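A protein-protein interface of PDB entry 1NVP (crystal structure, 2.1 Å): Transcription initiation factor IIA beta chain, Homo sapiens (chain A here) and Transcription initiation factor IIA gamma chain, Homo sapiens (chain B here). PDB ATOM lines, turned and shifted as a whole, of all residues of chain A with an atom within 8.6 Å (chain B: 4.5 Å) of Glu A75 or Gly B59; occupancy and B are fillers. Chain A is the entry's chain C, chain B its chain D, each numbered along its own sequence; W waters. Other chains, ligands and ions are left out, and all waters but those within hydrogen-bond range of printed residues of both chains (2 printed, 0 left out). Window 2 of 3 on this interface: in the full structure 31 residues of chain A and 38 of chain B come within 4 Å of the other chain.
The backbone carbonyl oxygen of Glu A75 lies within hydrogen-bond range of the backbone NH of Leu B61, at 2.7 Å. OD2 of Asp A73 lies within salt-bridge range of NH2 of Arg B58 (3.8 Å). The backbone carbonyl oxygen (O) of Asp A73 sits at hydrogen-bond distance from the backbone NH (N) of Gly B59 (2.9 Å).
Water W1 bridges O of Gly B59 (2.9 Å) and N of Glu A75 (3.3 Å). Water W2 bridges O of Leu B61 and OXT of Trp A76.
CD1 of Trp A49 touches CD2 of Leu B61 (3.6 Å). Ala A74 touches Gly B59. Ala A74 touches Leu B61 (CB to N, 3.6 Å). Ala A74 touches Leu B75. Gly B59 touches Glu A75. Ser B60 touches Glu A75 (CA to O, 3.5 Å). CA of Trp A76 touches O of Leu B61, 3.4 Å away.
The backbone carbonyl oxygen of Ser B60 sits at hydrogen-bond distance from the backbone NH of Asn B76 (2.9 Å). The backbone NH of Trp A49 sits at hydrogen-bond distance from the backbone carbonyl oxygen of Ala A74, 2.9 Å away. ND2 of Asn A47 is in hydrogen-bond range of O of Trp A76 (3.0 Å). NZ of Lys A48 is in salt-bridge range of OE2 of Glu A75 (2.7 Å).
Glu A75 touches just these residues of chain B: Gly B59 (3.5 Å), Ser B60 (3.5 Å) and Leu B61 (2.7 Å). Gly B59 touches three residues of chain A. Printed residues of chain A within 4 Å of Ser B60: Glu A75. Printed residues of chain B within 4 Å of Trp A76: Leu B61 (3.4 Å). Of the printed residues of chain B, Ala A74 touches Gly B59, Leu B61 and Leu B75. Of the printed residues of chain B, Trp A49 touches Leu B61. Of the printed residues of chain B, Asp A73 touches Arg B58 (3.2 Å) and Gly B59 (2.9 Å). Phe A51 touches none of the printed residues of chain B. Ser A45 touches none of the printed residues of chain B. The nearest residue of chain A that does not touch Gly B59 is Gly A72 (6.5 Å).
Of the 13 printed residues of chain A, 5 touch a printed residue of chain B. Printed residues of chain A that touch a printed residue of chain B: Trp A49, Asp A73, Ala A74, Glu A75 and Trp A76. Hydrophobic or aromatic side chains of chain A within 4 Å of the printed part of chain B: Trp A49, Ala A74 and Trp A76. Of the 8 printed residues of chain B, 5 touch a printed residue of chain A. Printed residues of chain B that touch a printed residue of chain A: Arg B58, Gly B59, Ser B60, Leu B61 and Leu B75. Among the printed residues, 10 pairs touch across the chains.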
ATOM      1  N   SER A  45     -14.358   1.772  -4.877  1.00  0.00           N
ATOM      2  CA  SER A  45     -15.530   1.129  -4.284  1.00  0.00           C
ATOM      3  C   SER A  45     -15.624  -0.178  -5.057  1.00  0.00           C
ATOM      4  O   SER A  45     -15.770  -0.178  -6.284  1.00  0.00           O
ATOM      5  CB  SER A  45     -16.780   1.957  -4.527  1.00  0.00           C
ATOM      6  OG  SER A  45     -16.865   3.000  -3.580  1.00  0.00           O
ATOM      7  N   LYS A  46     -15.543  -1.295  -4.347  1.00  0.00           N
ATOM      8  CA  LYS A  46     -15.584  -2.565  -5.056  1.00  0.00           C
ATOM      9  C   LYS A  46     -14.459  -2.458  -6.077  1.00  0.00           C
ATOM     10  O   LYS A  46     -13.337  -2.114  -5.708  1.00  0.00           O
ATOM     11  CB  LYS A  46     -16.944  -2.799  -5.758  1.00  0.00           C
ATOM     12  CG  LYS A  46     -18.089  -3.219  -4.815  1.00  0.00           C
ATOM     13  CD  LYS A  46     -17.937  -4.668  -4.374  1.00  0.00           C
ATOM     14  CE  LYS A  46     -18.992  -5.073  -3.343  1.00  0.00           C
ATOM     15  NZ  LYS A  46     -20.387  -5.069  -3.870  1.00  0.00           N
ATOM     16  N   ASN A  47     -14.744  -2.741  -7.344  1.00  0.00           N
ATOM     17  CA  ASN A  47     -13.706  -2.650  -8.365  1.00  0.00           C
ATOM     18  C   ASN A  47     -13.846  -1.387  -9.222  1.00  0.00           C
ATOM     19  O   ASN A  47     -13.414  -1.364 -10.372  1.00  0.00           O
ATOM     20  CB  ASN A  47     -13.732  -3.894  -9.253  1.00  0.00           C
ATOM     21  CG  ASN A  47     -14.900  -3.900 -10.211  1.00  0.00           C
ATOM     22  OD1 ASN A  47     -15.963  -3.364  -9.915  1.00  0.00           O
ATOM     23  ND2 ASN A  47     -14.709  -4.521 -11.368  1.00  0.00           N
ATOM     24  N   LYS A  48     -14.453  -0.344  -8.661  1.00  0.00           N
ATOM     25  CA  LYS A  48     -14.632   0.920  -9.373  1.00  0.00           C
ATOM     26  C   LYS A  48     -13.644   1.961  -8.845  1.00  0.00           C
ATOM     27  O   LYS A  48     -13.696   2.338  -7.671  1.00  0.00           O
ATOM     28  CB  LYS A  48     -16.048   1.468  -9.174  1.00  0.00           C
ATOM     29  CG  LYS A  48     -17.172   0.506  -9.486  1.00  0.00           C
ATOM     30  CD  LYS A  48     -17.112   0.011 -10.910  1.00  0.00           C
ATOM     31  CE  LYS A  48     -18.164  -1.054 -11.139  1.00  0.00           C
ATOM     32  NZ  LYS A  48     -17.792  -1.940 -12.267  1.00  0.00           N
ATOM     33  N   TRP A  49     -12.747   2.428  -9.705  1.00  0.00           N
ATOM     34  CA  TRP A  49     -11.782   3.435  -9.288  1.00  0.00           C
ATOM     35  C   TRP A  49     -12.069   4.774  -9.955  1.00  0.00           C
ATOM     36  O   TRP A  49     -12.519   4.823 -11.101  1.00  0.00           O
ATOM     37  CB  TRP A  49     -10.359   3.010  -9.646  1.00  0.00           C
ATOM     38  CG  TRP A  49      -9.842   1.820  -8.912  1.00  0.00           C
ATOM     39  CD1 TRP A  49     -10.247   0.524  -9.057  1.00  0.00           C
ATOM     40  CD2 TRP A  49      -8.772   1.803  -7.961  1.00  0.00           C
ATOM     41  NE1 TRP A  49      -9.488  -0.300  -8.261  1.00  0.00           N
ATOM     42  CE2 TRP A  49      -8.578   0.458  -7.576  1.00  0.00           C
ATOM     43  CE3 TRP A  49      -7.957   2.794  -7.398  1.00  0.00           C
ATOM     44  CZ2 TRP A  49      -7.600   0.080  -6.657  1.00  0.00           C
ATOM     45  CZ3 TRP A  49      -6.983   2.416  -6.482  1.00  0.00           C
ATOM     46  CH2 TRP A  49      -6.816   1.069  -6.120  1.00  0.00           C
ATOM     47  N   LYS A  50     -11.824   5.857  -9.225  1.00  0.00           N
ATOM     48  CA  LYS A  50     -12.005   7.204  -9.758  1.00  0.00           C
ATOM     49  C   LYS A  50     -10.718   7.950  -9.453  1.00  0.00           C
ATOM     50  O   LYS A  50     -10.215   7.892  -8.332  1.00  0.00           O
ATOM     51  CB  LYS A  50     -13.184   7.919  -9.098  1.00  0.00           C
ATOM     52  CG  LYS A  50     -14.540   7.331  -9.441  1.00  0.00           C
ATOM     53  CD  LYS A  50     -15.664   8.273  -9.033  1.00  0.00           C
ATOM     54  CE  LYS A  50     -17.016   7.576  -9.095  1.00  0.00           C
ATOM     55  NZ  LYS A  50     -18.151   8.525  -8.908  1.00  0.00           N
ATOM     56  N   PHE A  51     -10.176   8.643 -10.446  1.00  0.00           N
ATOM     57  CA  PHE A  51      -8.930   9.362 -10.235  1.00  0.00           C
ATOM     58  C   PHE A  51      -9.097  10.868 -10.376  1.00  0.00           C
ATOM     59  O   PHE A  51      -9.693  11.355 -11.337  1.00  0.00           O
ATOM     60  CB  PHE A  51      -7.863   8.887 -11.224  1.00  0.00           C
ATOM     61  CG  PHE A  51      -7.871   7.403 -11.473  1.00  0.00           C
ATOM     62  CD1 PHE A  51      -8.876   6.815 -12.239  1.00  0.00           C
ATOM     63  CD2 PHE A  51      -6.861   6.595 -10.963  1.00  0.00           C
ATOM     64  CE1 PHE A  51      -8.870   5.445 -12.496  1.00  0.00           C
ATOM     65  CE2 PHE A  51      -6.846   5.225 -11.214  1.00  0.00           C
ATOM     66  CZ  PHE A  51      -7.854   4.649 -11.983  1.00  0.00           C
ATOM     67  N   ILE A  71      -9.619  13.995 -14.688  1.00  0.00           N
ATOM     68  CA  ILE A  71     -10.555  13.148 -13.960  1.00  0.00           C
ATOM     69  C   ILE A  71     -10.796  11.885 -14.775  1.00  0.00           C
ATOM     70  O   ILE A  71     -11.145  11.955 -15.955  1.00  0.00           O
ATOM     71  CB  ILE A  71     -11.895  13.872 -13.732  1.00  0.00           C
ATOM     72  CG1 ILE A  71     -11.684  15.052 -12.783  1.00  0.00           C
ATOM     73  CG2 ILE A  71     -12.921  12.907 -13.164  1.00  0.00           C
ATOM     74  CD1 ILE A  71     -12.945  15.857 -12.513  1.00  0.00           C
ATOM     75  N   GLY A  72     -10.602  10.728 -14.146  1.00  0.00           N
ATOM     76  CA  GLY A  72     -10.797   9.480 -14.856  1.00  0.00           C
ATOM     77  C   GLY A  72     -11.592   8.405 -14.136  1.00  0.00           C
ATOM     78  O   GLY A  72     -11.810   8.475 -12.925  1.00  0.00           O
ATOM     79  N   ASP A  73     -12.019   7.402 -14.902  1.00  0.00           N
ATOM     80  CA  ASP A  73     -12.786   6.276 -14.381  1.00  0.00           C
ATOM     81  C   ASP A  73     -12.302   4.965 -14.977  1.00  0.00           C
ATOM     82  O   ASP A  73     -12.017   4.881 -16.171  1.00  0.00           O
ATOM     83  CB  ASP A  73     -14.273   6.432 -14.704  1.00  0.00           C
ATOM     84  CG  ASP A  73     -14.941   7.493 -13.864  1.00  0.00           C
ATOM     85  OD1 ASP A  73     -14.743   7.479 -12.631  1.00  0.00           O
ATOM     86  OD2 ASP A  73     -15.670   8.333 -14.431  1.00  0.00           O
ATOM     87  N   ALA A  74     -12.223   3.936 -14.144  1.00  0.00           N
ATOM     88  CA  ALA A  74     -11.784   2.636 -14.617  1.00  0.00           C
ATOM     89  C   ALA A  74     -12.255   1.495 -13.720  1.00  0.00           C
ATOM     90  O   ALA A  74     -12.406   1.657 -12.505  1.00  0.00           O
ATOM     91  CB  ALA A  74     -10.266   2.612 -14.732  1.00  0.00           C
ATOM     92  N   GLU A  75     -12.501   0.343 -14.336  1.00  0.00           N
ATOM     93  CA  GLU A  75     -12.912  -0.845 -13.605  1.00  0.00           C
ATOM     94  C   GLU A  75     -11.698  -1.741 -13.581  1.00  0.00           C
ATOM     95  O   GLU A  75     -10.978  -1.835 -14.573  1.00  0.00           O
ATOM     96  CB  GLU A  75     -14.053  -1.571 -14.313  1.00  0.00           C
ATOM     97  CG  GLU A  75     -15.397  -0.899 -14.195  1.00  0.00           C
ATOM     98  CD  GLU A  75     -16.519  -1.780 -14.707  1.00  0.00           C
ATOM     99  OE1 GLU A  75     -16.276  -2.988 -14.925  1.00  0.00           O
ATOM    100  OE2 GLU A  75     -17.645  -1.270 -14.879  1.00  0.00           O
ATOM    101  N   TRP A  76     -11.475  -2.404 -12.453  1.00  0.00           N
ATOM    102  CA  TRP A  76     -10.330  -3.285 -12.302  1.00  0.00           C
ATOM    103  C   TRP A  76     -10.732  -4.751 -12.466  1.00  0.00           C
ATOM    104  O   TRP A  76     -11.867  -5.084 -12.064  1.00  0.00           O
ATOM    105  CB  TRP A  76      -9.717  -3.065 -10.926  1.00  0.00           C
ATOM    106  CG  TRP A  76      -8.543  -3.907 -10.654  1.00  0.00           C
ATOM    107  CD1 TRP A  76      -7.266  -3.670 -11.042  1.00  0.00           C
ATOM    108  CD2 TRP A  76      -8.522  -5.130  -9.917  1.00  0.00           C
ATOM    109  NE1 TRP A  76      -6.439  -4.665 -10.592  1.00  0.00           N
ATOM    110  CE2 TRP A  76      -7.186  -5.580  -9.894  1.00  0.00           C
ATOM    111  CE3 TRP A  76      -9.505  -5.894  -9.266  1.00  0.00           C
ATOM    112  CZ2 TRP A  76      -6.797  -6.755  -9.252  1.00  0.00           C
ATOM    113  CZ3 TRP A  76      -9.123  -7.067  -8.623  1.00  0.00           C
ATOM    114  CH2 TRP A  76      -7.780  -7.486  -8.619  1.00  0.00           C
ATOM    115  OXT TRP A  76      -9.904  -5.546 -12.974  1.00  0.00           O
ATOM    116  N   ARG B  58     -11.255   7.557 -19.410  1.00  0.00           N
ATOM    117  CA  ARG B  58     -11.959   6.362 -18.976  1.00  0.00           C
ATOM    118  C   ARG B  58     -11.285   5.154 -19.605  1.00  0.00           C
ATOM    119  O   ARG B  58     -10.754   5.231 -20.715  1.00  0.00           O
ATOM    120  CB  ARG B  58     -13.426   6.428 -19.405  1.00  0.00           C
ATOM    121  CG  ARG B  58     -14.285   5.285 -18.890  1.00  0.00           C
ATOM    122  CD  ARG B  58     -15.717   5.427 -19.383  1.00  0.00           C
ATOM    123  NE  ARG B  58     -16.313   6.695 -18.971  1.00  0.00           N
ATOM    124  CZ  ARG B  58     -17.191   6.826 -17.981  1.00  0.00           C
ATOM    125  NH1 ARG B  58     -17.584   5.762 -17.293  1.00  0.00           N
ATOM    126  NH2 ARG B  58     -17.677   8.023 -17.679  1.00  0.00           N
ATOM    127  N   GLY B  59     -11.301   4.042 -18.883  1.00  0.00           N
ATOM    128  CA  GLY B  59     -10.688   2.830 -19.382  1.00  0.00           C
ATOM    129  C   GLY B  59     -10.781   1.731 -18.349  1.00  0.00           C
ATOM    130  O   GLY B  59     -11.486   1.868 -17.349  1.00  0.00           O
ATOM    131  N   SER B  60     -10.076   0.634 -18.587  1.00  0.00           N
ATOM    132  CA  SER B  60     -10.090  -0.473 -17.650  1.00  0.00           C
ATOM    133  C   SER B  60      -8.758  -0.465 -16.927  1.00  0.00           C
ATOM    134  O   SER B  60      -7.704  -0.315 -17.554  1.00  0.00           O
ATOM    135  CB  SER B  60     -10.272  -1.799 -18.386  1.00  0.00           C
ATOM    136  OG  SER B  60      -9.074  -2.192 -19.030  1.00  0.00           O
ATOM    137  N   LEU B  61      -8.807  -0.606 -15.607  1.00  0.00           N
ATOM    138  CA  LEU B  61      -7.598  -0.619 -14.803  1.00  0.00           C
ATOM    139  C   LEU B  61      -7.014  -2.024 -14.819  1.00  0.00           C
ATOM    140  O   LEU B  61      -7.679  -2.993 -14.453  1.00  0.00           O
ATOM    141  CB  LEU B  61      -7.914  -0.184 -13.368  1.00  0.00           C
ATOM    142  CG  LEU B  61      -6.720  -0.021 -12.427  1.00  0.00           C
ATOM    143  CD1 LEU B  61      -5.778   1.037 -12.989  1.00  0.00           C
ATOM    144  CD2 LEU B  61      -7.203   0.379 -11.031  1.00  0.00           C
ATOM    145  N   LEU B  75      -3.601   1.564 -17.323  1.00  0.00           N
ATOM    146  CA  LEU B  75      -4.944   1.430 -17.876  1.00  0.00           C
ATOM    147  C   LEU B  75      -4.857   0.851 -19.287  1.00  0.00           C
ATOM    148  O   LEU B  75      -3.846   1.022 -19.969  1.00  0.00           O
ATOM    149  CB  LEU B  75      -5.626   2.795 -17.958  1.00  0.00           C
ATOM    150  CG  LEU B  75      -6.055   3.598 -16.729  1.00  0.00           C
ATOM    151  CD1 LEU B  75      -7.384   3.086 -16.238  1.00  0.00           C
ATOM    152  CD2 LEU B  75      -4.995   3.529 -15.646  1.00  0.00           C
ATOM    153  N   ASN B  76      -5.910   0.162 -19.718  1.00  0.00           N
ATOM    154  CA  ASN B  76      -5.955  -0.409 -21.060  1.00  0.00           C
ATOM    155  C   ASN B  76      -7.174   0.157 -21.759  1.00  0.00           C
ATOM    156  O   ASN B  76      -8.159   0.504 -21.107  1.00  0.00           O
ATOM    157  CB  ASN B  76      -6.046  -1.933 -21.017  1.00  0.00           C
ATOM    158  CG  ASN B  76      -4.729  -2.586 -20.668  1.00  0.00           C
ATOM    159  OD1 ASN B  76      -4.609  -3.265 -19.650  1.00  0.00           O
ATOM    160  ND2 ASN B  76      -3.729  -2.390 -21.517  1.00  0.00           N
ATOM    161  N   ASP B  77      -7.095   0.269 -23.083  1.00  0.00           N
ATOM    162  CA  ASP B  77      -8.183   0.807 -23.894  1.00  0.00           C
ATOM    163  C   ASP B  77      -8.753   2.077 -23.284  1.00  0.00           C
ATOM    164  O   ASP B  77      -9.943   2.158 -22.983  1.00  0.00           O
ATOM    165  CB  ASP B  77      -9.292  -0.234 -24.053  1.00  0.00           C
ATOM    166  CG  ASP B  77      -8.761  -1.570 -24.526  1.00  0.00           C
ATOM    167  OD1 ASP B  77      -7.756  -1.578 -25.268  1.00  0.00           O
ATOM    168  OD2 ASP B  77      -9.353  -2.609 -24.165  1.00  0.00           O
ATOM    169  N   VAL B  78      -7.892   3.075 -23.121  1.00  0.00           N
ATOM    170  CA  VAL B  78      -8.287   4.347 -22.527  1.00  0.00           C
ATOM    171  C   VAL B  78      -8.741   5.383 -23.549  1.00  0.00           C
ATOM    172  O   VAL B  78      -8.380   5.323 -24.725  1.00  0.00           O
ATOM    173  CB  VAL B  78      -7.125   4.954 -21.726  1.00  0.00           C
ATOM    174  CG1 VAL B  78      -7.636   6.073 -20.836  1.00  0.00           C
ATOM    175  CG2 VAL B  78      -6.439   3.873 -20.920  1.00  0.00           C
HETATM  176  O   HOH W   1     -14.206   1.025 -17.077  1.00  0.00           O
HETATM  177  O   HOH W   2      -9.571  -4.688 -16.054  1.00  0.00           O
